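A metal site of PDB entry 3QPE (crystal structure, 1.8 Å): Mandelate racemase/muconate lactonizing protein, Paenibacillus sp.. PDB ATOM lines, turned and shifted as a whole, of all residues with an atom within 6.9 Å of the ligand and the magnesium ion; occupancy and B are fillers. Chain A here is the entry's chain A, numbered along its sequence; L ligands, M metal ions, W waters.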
ATOM      1  N   ALA A  32      26.027 -21.838  14.660  1.00  0.00           N
ATOM      2  CA  ALA A  32      24.679 -22.312  14.956  1.00  0.00           C
ATOM      3  C   ALA A  32      24.393 -22.316  16.452  1.00  0.00           C
ATOM      4  O   ALA A  32      25.313 -22.175  17.261  1.00  0.00           O
ATOM      5  CB  ALA A  32      24.497 -23.726  14.384  1.00  0.00           C
ATOM      6  N   ASN A  33      23.117 -22.426  16.817  1.00  0.00           N
ATOM      7  CA  ASN A  33      22.718 -22.699  18.188  1.00  0.00           C
ATOM      8  C   ASN A  33      21.882 -23.962  18.203  1.00  0.00           C
ATOM      9  O   ASN A  33      21.790 -24.646  17.179  1.00  0.00           O
ATOM     10  CB  ASN A  33      21.992 -21.502  18.864  1.00  0.00           C
ATOM     11  CG  ASN A  33      20.605 -21.250  18.298  1.00  0.00           C
ATOM     12  OD1 ASN A  33      20.051 -22.075  17.573  1.00  0.00           O
ATOM     13  ND2 ASN A  33      20.042 -20.086  18.625  1.00  0.00           N
ATOM     14  N   GLY A  34      21.283 -24.284  19.361  1.00  0.00           N
ATOM     15  CA  GLY A  34      20.589 -25.542  19.520  1.00  0.00           C
ATOM     16  C   GLY A  34      19.482 -25.814  18.509  1.00  0.00           C
ATOM     17  O   GLY A  34      19.220 -26.968  18.178  1.00  0.00           O
ATOM     18  N   ARG A  35      18.840 -24.759  18.003  1.00  0.00           N
ATOM     19  CA  ARG A  35      17.665 -24.936  17.142  1.00  0.00           C
ATOM     20  C   ARG A  35      17.840 -24.548  15.681  1.00  0.00           C
ATOM     21  O   ARG A  35      17.116 -25.068  14.827  1.00  0.00           O
ATOM     22  CB  ARG A  35      16.457 -24.185  17.712  1.00  0.00           C
ATOM     23  CG  ARG A  35      16.714 -22.702  18.048  1.00  0.00           C
ATOM     24  CD  ARG A  35      15.425 -22.013  18.550  1.00  0.00           C
ATOM     25  NE  ARG A  35      14.356 -22.091  17.554  1.00  0.00           N
ATOM     26  CZ  ARG A  35      14.157 -21.186  16.590  1.00  0.00           C
ATOM     27  NH1 ARG A  35      13.175 -21.365  15.724  1.00  0.00           N
ATOM     28  NH2 ARG A  35      14.946 -20.125  16.499  1.00  0.00           N
ATOM     29  N   ILE A  36      18.737 -23.618  15.390  1.00  0.00           N
ATOM     30  CA  ILE A  36      18.860 -23.110  14.018  1.00  0.00           C
ATOM     31  C   ILE A  36      20.306 -22.994  13.581  1.00  0.00           C
ATOM     32  O   ILE A  36      21.230 -23.278  14.345  1.00  0.00           O
ATOM     33  CB  ILE A  36      18.132 -21.751  13.830  1.00  0.00           C
ATOM     34  CG1 ILE A  36      18.738 -20.661  14.718  1.00  0.00           C
ATOM     35  CG2 ILE A  36      16.633 -21.905  14.128  1.00  0.00           C
ATOM     36  CD1 ILE A  36      18.184 -19.252  14.451  1.00  0.00           C
ATOM     37  N   GLY A  37      20.500 -22.585  12.332  1.00  0.00           N
ATOM     38  CA  GLY A  37      21.819 -22.560  11.729  1.00  0.00           C
ATOM     39  C   GLY A  37      22.705 -21.386  12.083  1.00  0.00           C
ATOM     40  O   GLY A  37      22.462 -20.655  13.043  1.00  0.00           O
ATOM     41  N   HIS A  39      24.487 -17.955  12.510  1.00  0.00           N
ATOM     42  CA  HIS A  39      23.897 -16.622  12.666  1.00  0.00           C
ATOM     43  C   HIS A  39      24.622 -15.586  11.830  1.00  0.00           C
ATOM     44  O   HIS A  39      24.032 -14.594  11.392  1.00  0.00           O
ATOM     45  CB  HIS A  39      23.876 -16.222  14.140  1.00  0.00           C
ATOM     46  CG  HIS A  39      22.859 -16.955  14.954  1.00  0.00           C
ATOM     47  ND1 HIS A  39      22.926 -18.314  15.187  1.00  0.00           N
ATOM     48  CD2 HIS A  39      21.748 -16.515  15.589  1.00  0.00           C
ATOM     49  CE1 HIS A  39      21.906 -18.676  15.939  1.00  0.00           C
ATOM     50  NE2 HIS A  39      21.172 -17.606  16.197  1.00  0.00           N
ATOM     51  N   TYR A 131      28.357 -10.013  30.377  1.00  0.00           N
ATOM     52  CA  TYR A 131      28.884 -11.328  30.019  1.00  0.00           C
ATOM     53  C   TYR A 131      29.010 -11.508  28.503  1.00  0.00           C
ATOM     54  O   TYR A 131      28.290 -10.869  27.721  1.00  0.00           O
ATOM     55  CB  TYR A 131      28.033 -12.442  30.629  1.00  0.00           C
ATOM     56  CG  TYR A 131      26.664 -12.618  30.026  1.00  0.00           C
ATOM     57  CD1 TYR A 131      26.491 -13.305  28.831  1.00  0.00           C
ATOM     58  CD2 TYR A 131      25.537 -12.126  30.659  1.00  0.00           C
ATOM     59  CE1 TYR A 131      25.230 -13.470  28.276  1.00  0.00           C
ATOM     60  CE2 TYR A 131      24.270 -12.298  30.115  1.00  0.00           C
ATOM     61  CZ  TYR A 131      24.123 -12.953  28.929  1.00  0.00           C
ATOM     62  OH  TYR A 131      22.865 -13.135  28.403  1.00  0.00           O
ATOM     63  N   THR A 133      28.328 -13.249  25.245  1.00  0.00           N
ATOM     64  CA  THR A 133      27.240 -14.094  24.769  1.00  0.00           C
ATOM     65  C   THR A 133      27.573 -14.783  23.447  1.00  0.00           C
ATOM     66  O   THR A 133      26.758 -15.511  22.887  1.00  0.00           O
ATOM     67  CB  THR A 133      25.913 -13.281  24.650  1.00  0.00           C
ATOM     68  OG1 THR A 133      24.779 -14.172  24.600  1.00  0.00           O
ATOM     69  CG2 THR A 133      25.913 -12.402  23.384  1.00  0.00           C
ATOM     70  N   TYR A 136      28.907 -19.544  20.340  1.00  0.00           N
ATOM     71  CA  TYR A 136      27.965 -20.393  19.631  1.00  0.00           C
ATOM     72  C   TYR A 136      28.571 -21.771  19.317  1.00  0.00           C
ATOM     73  O   TYR A 136      29.602 -22.122  19.877  1.00  0.00           O
ATOM     74  CB  TYR A 136      27.482 -19.662  18.372  1.00  0.00           C
ATOM     75  CG  TYR A 136      26.374 -18.695  18.708  1.00  0.00           C
ATOM     76  CD1 TYR A 136      26.592 -17.617  19.553  1.00  0.00           C
ATOM     77  CD2 TYR A 136      25.076 -18.889  18.215  1.00  0.00           C
ATOM     78  CE1 TYR A 136      25.546 -16.729  19.883  1.00  0.00           C
ATOM     79  CE2 TYR A 136      24.035 -18.024  18.552  1.00  0.00           C
ATOM     80  CZ  TYR A 136      24.279 -16.948  19.374  1.00  0.00           C
ATOM     81  OH  TYR A 136      23.228 -16.102  19.710  1.00  0.00           O
ATOM     82  N   LYS A 168      28.549 -16.893  28.400  1.00  0.00           N
ATOM     83  CA  LYS A 168      27.380 -17.735  28.168  1.00  0.00           C
ATOM     84  C   LYS A 168      27.607 -18.637  26.979  1.00  0.00           C
ATOM     85  O   LYS A 168      27.891 -18.187  25.875  1.00  0.00           O
ATOM     86  CB  LYS A 168      26.103 -16.908  27.984  1.00  0.00           C
ATOM     87  CG  LYS A 168      24.851 -17.769  27.841  1.00  0.00           C
ATOM     88  CD  LYS A 168      23.580 -16.957  28.060  1.00  0.00           C
ATOM     89  CE  LYS A 168      23.055 -16.353  26.761  1.00  0.00           C
ATOM     90  NZ  LYS A 168      21.952 -15.376  27.128  1.00  0.00           N
ATOM     91  N   LYS A 170      26.518 -21.619  24.321  1.00  0.00           N
ATOM     92  CA  LYS A 170      25.447 -22.350  23.672  1.00  0.00           C
ATOM     93  C   LYS A 170      25.660 -23.850  23.831  1.00  0.00           C
ATOM     94  O   LYS A 170      26.741 -24.345  23.539  1.00  0.00           O
ATOM     95  CB  LYS A 170      25.392 -21.995  22.186  1.00  0.00           C
ATOM     96  CG  LYS A 170      25.024 -20.546  21.930  1.00  0.00           C
ATOM     97  CD  LYS A 170      23.566 -20.278  22.338  1.00  0.00           C
ATOM     98  CE  LYS A 170      23.092 -18.884  21.887  1.00  0.00           C
ATOM     99  NZ  LYS A 170      22.735 -18.028  23.058  1.00  0.00           N
ATOM    100  N   ASP A 207      23.105 -22.100  27.670  1.00  0.00           N
ATOM    101  CA  ASP A 207      21.851 -21.748  27.006  1.00  0.00           C
ATOM    102  C   ASP A 207      21.543 -22.803  25.962  1.00  0.00           C
ATOM    103  O   ASP A 207      22.251 -22.931  24.965  1.00  0.00           O
ATOM    104  CB  ASP A 207      21.926 -20.330  26.406  1.00  0.00           C
ATOM    105  CG  ASP A 207      20.673 -19.935  25.656  1.00  0.00           C
ATOM    106  OD1 ASP A 207      19.743 -20.766  25.536  1.00  0.00           O
ATOM    107  OD2 ASP A 207      20.635 -18.788  25.133  1.00  0.00           O
ATOM    108  N   ALA A 208      20.486 -23.566  26.210  1.00  0.00           N
ATOM    109  CA  ALA A 208      20.188 -24.720  25.366  1.00  0.00           C
ATOM    110  C   ALA A 208      19.310 -24.389  24.176  1.00  0.00           C
ATOM    111  O   ALA A 208      19.121 -25.216  23.282  1.00  0.00           O
ATOM    112  CB  ALA A 208      19.555 -25.855  26.220  1.00  0.00           C
ATOM    113  N   ASN A 209      18.760 -23.181  24.151  1.00  0.00           N
ATOM    114  CA  ASN A 209      17.771 -22.844  23.128  1.00  0.00           C
ATOM    115  C   ASN A 209      16.745 -23.960  22.959  1.00  0.00           C
ATOM    116  O   ASN A 209      16.380 -24.337  21.841  1.00  0.00           O
ATOM    117  CB  ASN A 209      18.411 -22.455  21.799  1.00  0.00           C
ATOM    118  CG  ASN A 209      19.153 -21.132  21.884  1.00  0.00           C
ATOM    119  OD1 ASN A 209      20.379 -21.109  22.002  1.00  0.00           O
ATOM    120  ND2 ASN A 209      18.424 -20.021  21.841  1.00  0.00           N
ATOM    121  N   GLU A 233      19.732 -21.502  31.056  1.00  0.00           N
ATOM    122  CA  GLU A 233      18.817 -20.715  30.253  1.00  0.00           C
ATOM    123  C   GLU A 233      18.127 -21.548  29.179  1.00  0.00           C
ATOM    124  O   GLU A 233      18.788 -22.233  28.394  1.00  0.00           O
ATOM    125  CB  GLU A 233      19.585 -19.545  29.619  1.00  0.00           C
ATOM    126  CG  GLU A 233      18.860 -18.823  28.480  1.00  0.00           C
ATOM    127  CD  GLU A 233      19.524 -17.507  28.118  1.00  0.00           C
ATOM    128  OE1 GLU A 233      20.418 -17.032  28.834  1.00  0.00           O
ATOM    129  OE2 GLU A 233      19.105 -16.922  27.119  1.00  0.00           O
ATOM    130  N   GLU A 234      16.805 -21.509  29.151  1.00  0.00           N
ATOM    131  CA  GLU A 234      16.015 -22.229  28.142  1.00  0.00           C
ATOM    132  C   GLU A 234      16.451 -23.679  27.903  1.00  0.00           C
ATOM    133  O   GLU A 234      16.684 -24.085  26.766  1.00  0.00           O
ATOM    134  CB  GLU A 234      15.987 -21.463  26.818  1.00  0.00           C
ATOM    135  CG  GLU A 234      15.314 -20.093  26.917  1.00  0.00           C
ATOM    136  CD  GLU A 234      14.630 -19.675  25.599  1.00  0.00           C
ATOM    137  OE1 GLU A 234      15.300 -19.580  24.560  1.00  0.00           O
ATOM    138  OE2 GLU A 234      13.420 -19.453  25.606  1.00  0.00           O
ATOM    139  N   GLU A 263      12.866 -15.255  26.789  1.00  0.00           N
ATOM    140  CA  GLU A 263      13.041 -14.649  25.452  1.00  0.00           C
ATOM    141  C   GLU A 263      12.019 -15.174  24.433  1.00  0.00           C
ATOM    142  O   GLU A 263      11.411 -16.232  24.633  1.00  0.00           O
ATOM    143  CB  GLU A 263      14.476 -14.846  24.932  1.00  0.00           C
ATOM    144  CG  GLU A 263      14.738 -16.239  24.387  1.00  0.00           C
ATOM    145  CD  GLU A 263      16.195 -16.439  24.026  1.00  0.00           C
ATOM    146  OE1 GLU A 263      16.487 -16.793  22.856  1.00  0.00           O
ATOM    147  OE2 GLU A 263      17.054 -16.232  24.911  1.00  0.00           O
ATOM    148  N   GLN A 283      13.943 -12.951  31.131  1.00  0.00           N
ATOM    149  CA  GLN A 283      14.814 -12.518  30.031  1.00  0.00           C
ATOM    150  C   GLN A 283      14.108 -11.906  28.807  1.00  0.00           C
ATOM    151  O   GLN A 283      14.580 -12.035  27.669  1.00  0.00           O
ATOM    152  CB  GLN A 283      15.682 -13.719  29.600  1.00  0.00           C
ATOM    153  CG  GLN A 283      16.550 -14.235  30.721  1.00  0.00           C
ATOM    154  CD  GLN A 283      17.498 -15.328  30.261  1.00  0.00           C
ATOM    155  OE1 GLN A 283      17.072 -16.351  29.731  1.00  0.00           O
ATOM    156  NE2 GLN A 283      18.788 -15.123  30.482  1.00  0.00           N
ATOM    157  N   HIS A 311      17.169  -9.897  27.510  1.00  0.00           N
ATOM    158  CA  HIS A 311      17.790 -10.522  26.351  1.00  0.00           C
ATOM    159  C   HIS A 311      18.213  -9.435  25.367  1.00  0.00           C
ATOM    160  O   HIS A 311      17.477  -8.472  25.137  1.00  0.00           O
ATOM    161  CB  HIS A 311      16.785 -11.451  25.662  1.00  0.00           C
ATOM    162  CG  HIS A 311      17.222 -11.936  24.308  1.00  0.00           C
ATOM    163  ND1 HIS A 311      17.104 -11.175  23.167  1.00  0.00           N
ATOM    164  CD2 HIS A 311      17.753 -13.126  23.922  1.00  0.00           C
ATOM    165  CE1 HIS A 311      17.550 -11.861  22.135  1.00  0.00           C
ATOM    166  NE2 HIS A 311      17.966 -13.038  22.555  1.00  0.00           N
ATOM    167  N   CYS A 312      19.404  -9.585  24.813  1.00  0.00           N
ATOM    168  CA  CYS A 312      19.845  -8.687  23.756  1.00  0.00           C
ATOM    169  C   CYS A 312      20.753  -9.483  22.825  1.00  0.00           C
ATOM    170  O   CYS A 312      21.846  -9.890  23.209  1.00  0.00           O
ATOM    171  CB  CYS A 312      20.599  -7.495  24.332  1.00  0.00           C
ATOM    172  SG  CYS A 312      21.176  -6.345  23.071  1.00  0.00           S
ATOM    173  N   TYR A 313      20.277  -9.724  21.624  1.00  0.00           N
ATOM    174  CA  TYR A 313      21.081 -10.362  20.602  1.00  0.00           C
ATOM    175  C   TYR A 313      20.408 -10.039  19.283  1.00  0.00           C
ATOM    176  O   TYR A 313      19.187 -10.132  19.156  1.00  0.00           O
ATOM    177  CB  TYR A 313      21.176 -11.887  20.804  1.00  0.00           C
ATOM    178  CG  TYR A 313      22.276 -12.471  19.952  1.00  0.00           C
ATOM    179  CD1 TYR A 313      23.590 -12.445  20.384  1.00  0.00           C
ATOM    180  CD2 TYR A 313      22.013 -12.999  18.704  1.00  0.00           C
ATOM    181  CE1 TYR A 313      24.635 -12.955  19.587  1.00  0.00           C
ATOM    182  CE2 TYR A 313      23.035 -13.513  17.899  1.00  0.00           C
ATOM    183  CZ  TYR A 313      24.337 -13.487  18.353  1.00  0.00           C
ATOM    184  OH  TYR A 313      25.363 -13.989  17.570  1.00  0.00           O
ATOM    185  N   GLY A 314      21.204  -9.600  18.304  1.00  0.00           N
ATOM    186  CA  GLY A 314      20.672  -9.260  17.010  1.00  0.00           C
ATOM    187  C   GLY A 314      20.465  -7.768  16.849  1.00  0.00           C
ATOM    188  O   GLY A 314      20.059  -7.300  15.785  1.00  0.00           O
ATOM    189  N   GLU A 336      23.895  -8.326  28.463  1.00  0.00           N
ATOM    190  CA  GLU A 336      24.277  -9.362  27.514  1.00  0.00           C
ATOM    191  C   GLU A 336      25.136  -8.754  26.393  1.00  0.00           C
ATOM    192  O   GLU A 336      24.650  -7.943  25.608  1.00  0.00           O
ATOM    193  CB  GLU A 336      23.045 -10.079  26.938  1.00  0.00           C
ATOM    194  CG  GLU A 336      23.413 -11.286  26.074  1.00  0.00           C
ATOM    195  CD  GLU A 336      22.209 -12.096  25.616  1.00  0.00           C
ATOM    196  OE1 GLU A 336      21.066 -11.685  25.898  1.00  0.00           O
ATOM    197  OE2 GLU A 336      22.410 -13.144  24.973  1.00  0.00           O
HETATM  198  O1  LIG L   1      17.977 -14.490  17.656  1.00  0.00           O
HETATM  199  O2  LIG L   1      18.961 -17.133  17.677  1.00  0.00           O
HETATM  200  O3  LIG L   1      19.035 -17.275  22.762  1.00  0.00           O
HETATM  201  O4  LIG L   1      20.189 -15.733  24.783  1.00  0.00           O
HETATM  202  C1  LIG L   1      18.517 -14.969  18.662  1.00  0.00           C
HETATM  203  C2  LIG L   1      19.501 -16.151  18.583  1.00  0.00           C
HETATM  204  C3  LIG L   1      19.756 -16.814  19.960  1.00  0.00           C
HETATM  205  C4  LIG L   1      20.072 -15.811  21.100  1.00  0.00           C
HETATM  206  C5  LIG L   1      20.173 -16.456  22.489  1.00  0.00           C
HETATM  207  C6  LIG L   1      20.454 -15.409  23.597  1.00  0.00           C
HETATM  208  O5  LIG L   1      20.851 -17.735  19.844  1.00  0.00           O
HETATM  209  O6  LIG L   1      19.026 -14.842  21.164  1.00  0.00           O
HETATM  210  O7  LIG L   1      20.925 -14.318  23.216  1.00  0.00           O
HETATM  211 MG    MG M   1      18.871 -17.466  25.125  1.00  0.00          MG
HETATM  212  O   HOH W   1      17.613 -19.232  24.796  1.00  0.00           O
HETATM  213  O   HOH W   2      23.634 -15.221  22.407  1.00  0.00           O
HETATM  214  O   HOH W   3      17.013 -19.140  18.202  1.00  0.00           O
HETATM  215  O   HOH W   4      19.301 -13.654  27.184  1.00  0.00           O
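A ring nitrogen (NE2) of His 311 is in hydrogen-bond range of an oxygen (O6) of the ligand (2.5 Å).
An oxygen (O7) of the ligand sits close to the side-chain carboxylate (OE2) of Glu 336.
NE2 of His 39 sits at hydrogen-bond distance from O2 of the ligand (2.7 Å).
ND2 of Asn 33 sits at hydrogen-bond distance from O5 of the ligand (2.8 Å).
The side-chain hydroxyl of Tyr 136 sits at hydrogen-bond distance from an oxygen (O5) of the ligand (2.9 Å).
The side-chain amino group (NZ) of Lys 168 sits close to an oxygen (O4) of the ligand, at 3.0 Å.
The side-chain amide nitrogen of Asn 209 lies close to an oxygen (O3) of the ligand (3.0 Å).
An oxygen (O4) of the ligand sits close to the side-chain amino group (NZ) of Lys 170, 3.8 Å away.
OE1 of Glu 233 lies within hydrogen-bond range of NE2 of Gln 283 (3.0 Å).
O of Glu 233 lies within hydrogen-bond range of N of Ala 208, at 3.1 Å.
The side-chain carboxylate of Asp 207 sits close to the side-chain amino group of Lys 170 (3.0 Å).
NZ of Lys 168 is in salt-bridge range of OE2 of Glu 336, 3.1 Å away.
The side-chain hydroxyl of Thr 133 sits at hydrogen-bond distance from the side-chain carboxylate of Glu 336 (2.6 Å).
The side-chain carboxylate (OE1) of Glu 336 lies within hydrogen-bond range of the backbone NH (N) of Cys 312 (2.9 Å).
The backbone NH (N) of Arg 35 is in hydrogen-bond range of the side-chain amide oxygen (OD1) of Asn 33, at 3.0 Å.
The backbone carbonyl oxygen of Glu 234 sits at hydrogen-bond distance from the backbone NH of Asn 209, at 3.5 Å.
Merely in contact with the ligand: Ile 36 and Tyr 313.
Within 4 Å of the ligand: Asn 33, Ile 36, His 39, Tyr 136, Lys 168, Lys 170, Asp 207, Asn 209, Glu 233, Glu 263, His 311, Tyr 313 and Glu 336.
The nearest printed residue that does not touch the ligand is Thr 133 (4.1 Å).
Of the 24 residues printed, 3 come within 4 Å of the magnesium ion.
The nearest printed residue that does not touch the magnesium ion is Asn 209 (4.2 Å).
The magnesium ion is bound by OE2 of Glu 233 (2.1 Å), water W1 (2.2 Å), O4 of the ligand (2.2 Å), OD2 of Asp 207 (2.2 Å), OE2 of Glu 263 (2.2 Å) and O3 of the ligand (2.4 Å).
The magnesium ion has six donor atoms within binding distance.
Water W1 lies within hydrogen-bond range of the side-chain carboxylate (OD1) of Asp 207 (2.7 Å), the side-chain amide nitrogen (ND2) of Asn 209 (3.2 Å) and the side-chain carboxylate (OE1) of Glu 263 (3.3 Å).
Water W3 lies within hydrogen-bond range of an oxygen (O2) of the ligand (2.8 Å), the guanidinium group of Arg 35 (2.9 Å) and the side-chain amide nitrogen of Asn 33 (3.2 Å).
Water W2 lies within hydrogen-bond range of the side-chain hydroxyl of Thr 133 (2.7 Å), the side-chain hydroxyl of Tyr 136 (2.9 Å), an oxygen (O7) of the ligand (3.0 Å) and the side-chain amino group of Lys 170 (3.0 Å).
Water W4 lies within hydrogen-bond range of OE1 of Glu 336 and NZ of Lys 168.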
